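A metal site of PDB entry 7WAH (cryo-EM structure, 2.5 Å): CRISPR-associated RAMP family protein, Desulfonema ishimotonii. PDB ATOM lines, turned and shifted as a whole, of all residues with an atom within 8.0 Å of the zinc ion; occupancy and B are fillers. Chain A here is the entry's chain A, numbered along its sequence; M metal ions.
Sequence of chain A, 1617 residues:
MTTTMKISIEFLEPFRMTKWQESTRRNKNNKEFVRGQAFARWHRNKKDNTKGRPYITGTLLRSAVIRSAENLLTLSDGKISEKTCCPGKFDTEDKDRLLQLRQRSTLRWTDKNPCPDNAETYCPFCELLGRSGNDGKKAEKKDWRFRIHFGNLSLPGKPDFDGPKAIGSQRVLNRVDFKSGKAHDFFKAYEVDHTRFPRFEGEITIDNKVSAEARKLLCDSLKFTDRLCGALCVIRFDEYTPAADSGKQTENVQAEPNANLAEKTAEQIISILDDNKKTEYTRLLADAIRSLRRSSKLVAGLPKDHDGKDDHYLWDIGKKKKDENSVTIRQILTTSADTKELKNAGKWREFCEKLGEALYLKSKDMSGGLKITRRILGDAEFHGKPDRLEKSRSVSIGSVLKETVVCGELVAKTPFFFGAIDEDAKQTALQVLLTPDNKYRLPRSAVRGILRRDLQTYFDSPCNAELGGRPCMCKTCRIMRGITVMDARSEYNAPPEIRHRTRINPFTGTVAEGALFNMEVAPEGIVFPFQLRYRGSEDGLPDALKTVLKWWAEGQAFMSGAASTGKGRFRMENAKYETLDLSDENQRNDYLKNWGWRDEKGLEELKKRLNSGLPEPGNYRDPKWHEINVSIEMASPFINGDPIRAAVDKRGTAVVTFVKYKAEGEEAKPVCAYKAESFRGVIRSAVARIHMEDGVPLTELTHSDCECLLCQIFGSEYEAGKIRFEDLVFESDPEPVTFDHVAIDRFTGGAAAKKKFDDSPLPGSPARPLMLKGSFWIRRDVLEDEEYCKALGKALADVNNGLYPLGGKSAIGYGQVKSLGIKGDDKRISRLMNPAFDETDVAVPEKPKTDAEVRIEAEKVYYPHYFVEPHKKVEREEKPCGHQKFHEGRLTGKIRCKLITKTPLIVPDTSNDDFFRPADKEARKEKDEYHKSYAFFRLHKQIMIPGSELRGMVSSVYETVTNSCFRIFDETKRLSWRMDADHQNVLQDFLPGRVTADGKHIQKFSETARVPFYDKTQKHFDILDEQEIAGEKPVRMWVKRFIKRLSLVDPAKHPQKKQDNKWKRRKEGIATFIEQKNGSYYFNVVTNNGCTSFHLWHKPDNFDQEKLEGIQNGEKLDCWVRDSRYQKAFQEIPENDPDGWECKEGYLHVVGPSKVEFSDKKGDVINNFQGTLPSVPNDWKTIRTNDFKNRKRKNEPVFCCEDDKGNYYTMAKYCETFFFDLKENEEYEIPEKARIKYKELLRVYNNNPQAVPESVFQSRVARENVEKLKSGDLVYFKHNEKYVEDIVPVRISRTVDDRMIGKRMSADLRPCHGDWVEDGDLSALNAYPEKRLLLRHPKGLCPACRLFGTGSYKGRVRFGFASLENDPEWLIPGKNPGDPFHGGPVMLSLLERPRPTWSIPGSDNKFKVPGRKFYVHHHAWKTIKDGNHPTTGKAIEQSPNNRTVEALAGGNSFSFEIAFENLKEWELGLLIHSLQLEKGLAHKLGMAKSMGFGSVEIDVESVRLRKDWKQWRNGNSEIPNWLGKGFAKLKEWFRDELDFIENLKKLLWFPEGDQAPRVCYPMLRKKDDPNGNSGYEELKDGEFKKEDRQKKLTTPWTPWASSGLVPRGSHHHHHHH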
ATOM      1  N   ARG A 684      11.424 -20.400  -5.366  1.00  0.00           N
ATOM      2  CA  ARG A 684      10.393 -19.455  -5.789  1.00  0.00           C
ATOM      3  C   ARG A 684       9.024 -20.125  -5.851  1.00  0.00           C
ATOM      4  O   ARG A 684       8.014 -19.530  -5.437  1.00  0.00           O
ATOM      5  CB  ARG A 684      10.776 -18.861  -7.141  1.00  0.00           C
ATOM      6  CG  ARG A 684       9.697 -18.032  -7.807  1.00  0.00           C
ATOM      7  CD  ARG A 684      10.294 -17.184  -8.910  1.00  0.00           C
ATOM      8  NE  ARG A 684       9.304 -16.753  -9.881  1.00  0.00           N
ATOM      9  CZ  ARG A 684       9.510 -15.820 -10.802  1.00  0.00           C
ATOM     10  NH1 ARG A 684      10.663 -15.162 -10.870  1.00  0.00           N
ATOM     11  NH2 ARG A 684       8.552 -15.543 -11.672  1.00  0.00           N
ATOM     12  N   GLU A 693      -2.130 -13.121  -3.468  1.00  0.00           N
ATOM     13  CA  GLU A 693      -2.355 -11.684  -3.415  1.00  0.00           C
ATOM     14  C   GLU A 693      -3.751 -11.362  -3.952  1.00  0.00           C
ATOM     15  O   GLU A 693      -4.152 -11.878  -4.994  1.00  0.00           O
ATOM     16  CB  GLU A 693      -1.303 -10.926  -4.233  1.00  0.00           C
ATOM     17  CG  GLU A 693      -1.417  -9.420  -4.124  1.00  0.00           C
ATOM     18  CD  GLU A 693      -1.212  -8.921  -2.697  1.00  0.00           C
ATOM     19  OE1 GLU A 693      -0.344  -9.474  -1.993  1.00  0.00           O
ATOM     20  OE2 GLU A 693      -1.931  -7.990  -2.289  1.00  0.00           O
ATOM     21  N   LEU A 698       0.209 -16.035  -6.379  1.00  0.00           N
ATOM     22  CA  LEU A 698       1.228 -15.250  -7.070  1.00  0.00           C
ATOM     23  C   LEU A 698       1.543 -15.817  -8.444  1.00  0.00           C
ATOM     24  O   LEU A 698       1.923 -15.075  -9.354  1.00  0.00           O
ATOM     25  CB  LEU A 698       2.498 -15.179  -6.211  1.00  0.00           C
ATOM     26  CG  LEU A 698       2.299 -14.718  -4.768  1.00  0.00           C
ATOM     27  CD1 LEU A 698       3.621 -14.650  -4.034  1.00  0.00           C
ATOM     28  CD2 LEU A 698       1.592 -13.376  -4.722  1.00  0.00           C
ATOM     29  N   LEU A 701      -0.800 -14.473 -11.231  1.00  0.00           N
ATOM     30  CA  LEU A 701      -0.628 -13.067 -11.538  1.00  0.00           C
ATOM     31  C   LEU A 701       0.280 -12.883 -12.758  1.00  0.00           C
ATOM     32  O   LEU A 701       1.237 -13.639 -12.960  1.00  0.00           O
ATOM     33  CB  LEU A 701      -0.046 -12.314 -10.340  1.00  0.00           C
ATOM     34  CG  LEU A 701      -0.846 -12.360  -9.039  1.00  0.00           C
ATOM     35  CD1 LEU A 701      -0.145 -11.572  -7.955  1.00  0.00           C
ATOM     36  CD2 LEU A 701      -2.252 -11.825  -9.264  1.00  0.00           C
ATOM     37  N   THR A 702      -0.038 -11.873 -13.562  1.00  0.00           N
ATOM     38  CA  THR A 702       0.791 -11.574 -14.731  1.00  0.00           C
ATOM     39  C   THR A 702       2.162 -11.051 -14.317  1.00  0.00           C
ATOM     40  O   THR A 702       3.112 -11.075 -15.109  1.00  0.00           O
ATOM     41  CB  THR A 702       0.084 -10.579 -15.647  1.00  0.00           C
ATOM     42  OG1 THR A 702      -0.140  -9.352 -14.943  1.00  0.00           O
ATOM     43  CG2 THR A 702      -1.247 -11.136 -16.123  1.00  0.00           C
ATOM     44  N   HIS A 703       2.282 -10.570 -13.080  1.00  0.00           N
ATOM     45  CA  HIS A 703       3.539 -10.040 -12.539  1.00  0.00           C
ATOM     46  C   HIS A 703       4.101  -8.909 -13.389  1.00  0.00           C
ATOM     47  O   HIS A 703       5.320  -8.815 -13.580  1.00  0.00           O
ATOM     48  CB  HIS A 703       4.577 -11.145 -12.353  1.00  0.00           C
ATOM     49  CG  HIS A 703       4.341 -12.000 -11.146  1.00  0.00           C
ATOM     50  ND1 HIS A 703       4.415 -11.507  -9.866  1.00  0.00           N
ATOM     51  CD2 HIS A 703       4.014 -13.310 -11.030  1.00  0.00           C
ATOM     52  CE1 HIS A 703       4.158 -12.480  -9.005  1.00  0.00           C
ATOM     53  NE2 HIS A 703       3.908 -13.584  -9.687  1.00  0.00           N
ATOM     54  N   SER A 704       3.229  -8.039 -13.892  1.00  0.00           N
ATOM     55  CA  SER A 704       3.633  -6.867 -14.661  1.00  0.00           C
ATOM     56  C   SER A 704       3.231  -5.604 -13.907  1.00  0.00           C
ATOM     57  O   SER A 704       2.045  -5.397 -13.622  1.00  0.00           O
ATOM     58  CB  SER A 704       2.990  -6.886 -16.046  1.00  0.00           C
ATOM     59  OG  SER A 704       3.193  -5.664 -16.722  1.00  0.00           O
ATOM     60  N   ASP A 705       4.225  -4.772 -13.586  1.00  0.00           N
ATOM     61  CA  ASP A 705       4.005  -3.488 -12.934  1.00  0.00           C
ATOM     62  C   ASP A 705       3.217  -3.648 -11.637  1.00  0.00           C
ATOM     63  O   ASP A 705       2.201  -2.984 -11.412  1.00  0.00           O
ATOM     64  CB  ASP A 705       3.311  -2.500 -13.876  1.00  0.00           C
ATOM     65  CG  ASP A 705       3.429  -1.063 -13.427  1.00  0.00           C
ATOM     66  OD1 ASP A 705       4.034  -0.814 -12.369  1.00  0.00           O
ATOM     67  OD2 ASP A 705       2.933  -0.166 -14.145  1.00  0.00           O
ATOM     68  N   CYS A 706       3.685  -4.539 -10.772  1.00  0.00           N
ATOM     69  CA  CYS A 706       3.020  -4.818  -9.502  1.00  0.00           C
ATOM     70  C   CYS A 706       4.042  -4.843  -8.377  1.00  0.00           C
ATOM     71  O   CYS A 706       5.243  -4.951  -8.593  1.00  0.00           O
ATOM     72  CB  CYS A 706       2.239  -6.132  -9.546  1.00  0.00           C
ATOM     73  SG  CYS A 706       3.217  -7.578 -10.006  1.00  0.00           S
ATOM     74  N   GLU A 707       3.524  -4.731  -7.147  1.00  0.00           N
ATOM     75  CA  GLU A 707       4.339  -4.715  -5.942  1.00  0.00           C
ATOM     76  C   GLU A 707       4.170  -5.989  -5.114  1.00  0.00           C
ATOM     77  O   GLU A 707       4.379  -5.961  -3.895  1.00  0.00           O
ATOM     78  CB  GLU A 707       4.013  -3.485  -5.092  1.00  0.00           C
ATOM     79  CG  GLU A 707       2.566  -3.430  -4.609  1.00  0.00           C
ATOM     80  CD  GLU A 707       2.311  -2.283  -3.662  1.00  0.00           C
ATOM     81  OE1 GLU A 707       3.239  -1.486  -3.410  1.00  0.00           O
ATOM     82  OE2 GLU A 707       1.176  -2.170  -3.155  1.00  0.00           O
ATOM     83  N   CYS A 708       3.784  -7.087  -5.751  1.00  0.00           N
ATOM     84  CA  CYS A 708       3.476  -8.301  -5.002  1.00  0.00           C
ATOM     85  C   CYS A 708       4.728  -8.891  -4.382  1.00  0.00           C
ATOM     86  O   CYS A 708       5.866  -8.565  -4.748  1.00  0.00           O
ATOM     87  CB  CYS A 708       2.796  -9.329  -5.917  1.00  0.00           C
ATOM     88  SG  CYS A 708       3.861 -10.062  -7.169  1.00  0.00           S
ATOM     89  N   LEU A 709       4.508  -9.791  -3.421  1.00  0.00           N
ATOM     90  CA  LEU A 709       5.603 -10.341  -2.626  1.00  0.00           C
ATOM     91  C   LEU A 709       6.646 -11.022  -3.498  1.00  0.00           C
ATOM     92  O   LEU A 709       7.858 -10.888  -3.261  1.00  0.00           O
ATOM     93  CB  LEU A 709       5.028 -11.314  -1.589  1.00  0.00           C
ATOM     94  CG  LEU A 709       5.914 -11.793  -0.456  1.00  0.00           C
ATOM     95  CD1 LEU A 709       5.575 -11.063   0.829  1.00  0.00           C
ATOM     96  CD2 LEU A 709       5.776 -13.296  -0.298  1.00  0.00           C
ATOM     97  N   LEU A 710       6.191 -11.773  -4.504  1.00  0.00           N
ATOM     98  CA  LEU A 710       7.109 -12.519  -5.348  1.00  0.00           C
ATOM     99  C   LEU A 710       8.035 -11.586  -6.123  1.00  0.00           C
ATOM    100  O   LEU A 710       9.229 -11.867  -6.264  1.00  0.00           O
ATOM    101  CB  LEU A 710       6.331 -13.415  -6.309  1.00  0.00           C
ATOM    102  CG  LEU A 710       7.119 -14.591  -6.905  1.00  0.00           C
ATOM    103  CD1 LEU A 710       7.267 -15.700  -5.864  1.00  0.00           C
ATOM    104  CD2 LEU A 710       6.466 -15.104  -8.171  1.00  0.00           C
ATOM    105  N   CYS A 711       7.504 -10.478  -6.647  1.00  0.00           N
ATOM    106  CA  CYS A 711       8.350  -9.527  -7.364  1.00  0.00           C
ATOM    107  C   CYS A 711       9.311  -8.818  -6.424  1.00  0.00           C
ATOM    108  O   CYS A 711      10.449  -8.525  -6.791  1.00  0.00           O
ATOM    109  CB  CYS A 711       7.496  -8.517  -8.114  1.00  0.00           C
ATOM    110  SG  CYS A 711       6.648  -9.188  -9.568  1.00  0.00           S
ATOM    111  N   GLN A 712       8.865  -8.528  -5.192  1.00  0.00           N
ATOM    112  CA  GLN A 712       9.729  -7.875  -4.226  1.00  0.00           C
ATOM    113  C   GLN A 712      10.914  -8.760  -3.861  1.00  0.00           C
ATOM    114  O   GLN A 712      12.052  -8.292  -3.735  1.00  0.00           O
ATOM    115  CB  GLN A 712       8.936  -7.494  -2.978  1.00  0.00           C
ATOM    116  CG  GLN A 712       7.767  -6.562  -3.245  1.00  0.00           C
ATOM    117  CD  GLN A 712       8.202  -5.231  -3.838  1.00  0.00           C
ATOM    118  OE1 GLN A 712       7.521  -4.675  -4.704  1.00  0.00           O
ATOM    119  NE2 GLN A 712       9.327  -4.707  -3.363  1.00  0.00           N
ATOM    120  N   GLY A 715      12.141 -10.445  -7.971  1.00  0.00           N
ATOM    121  CA  GLY A 715      12.218  -9.631  -9.164  1.00  0.00           C
ATOM    122  C   GLY A 715      11.333 -10.151 -10.277  1.00  0.00           C
ATOM    123  O   GLY A 715      10.692 -11.202 -10.183  1.00  0.00           O
ATOM    124  N   SER A 716      11.303  -9.390 -11.368  1.00  0.00           N
ATOM    125  CA  SER A 716      10.470  -9.718 -12.517  1.00  0.00           C
ATOM    126  C   SER A 716      11.112  -9.156 -13.772  1.00  0.00           C
ATOM    127  O   SER A 716      12.253  -8.701 -13.757  1.00  0.00           O
ATOM    128  CB  SER A 716       9.047  -9.194 -12.326  1.00  0.00           C
ATOM    129  OG  SER A 716       8.381  -9.890 -11.284  1.00  0.00           O
ATOM    130  N   GLU A 719      12.204  -5.360 -13.051  1.00  0.00           N
ATOM    131  CA  GLU A 719      13.274  -4.961 -12.143  1.00  0.00           C
ATOM    132  C   GLU A 719      14.069  -6.189 -11.715  1.00  0.00           C
ATOM    133  O   GLU A 719      13.590  -7.326 -11.790  1.00  0.00           O
ATOM    134  CB  GLU A 719      12.696  -4.257 -10.902  1.00  0.00           C
ATOM    135  CG  GLU A 719      11.673  -5.088 -10.151  1.00  0.00           C
ATOM    136  CD  GLU A 719      11.099  -4.367  -8.947  1.00  0.00           C
ATOM    137  OE1 GLU A 719      11.574  -3.257  -8.643  1.00  0.00           O
ATOM    138  OE2 GLU A 719      10.184  -4.919  -8.313  1.00  0.00           O
HETATM  139 ZN    ZN M   1       4.373  -9.484  -9.349  1.00  0.00          ZN
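SG of Cys 711 sits close to OG of Ser 716 (2.5 Å).
The backbone carbonyl oxygen (O) of Leu 698 sits at hydrogen-bond distance from a ring nitrogen (NE2) of His 703.
Within 4 Å of the zinc ion: His 703, Cys 706, Cys 708 and Cys 711.
The zinc ion is bound by a ring nitrogen (ND1) of His 703 (2.1 Å), the side-chain sulfur (SG) of Cys 711 (2.3 Å), the side-chain sulfur (SG) of Cys 708 (2.3 Å) and the side-chain sulfur (SG) of Cys 706 (2.3 Å).
The zinc ion has four donor atoms within binding distance.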
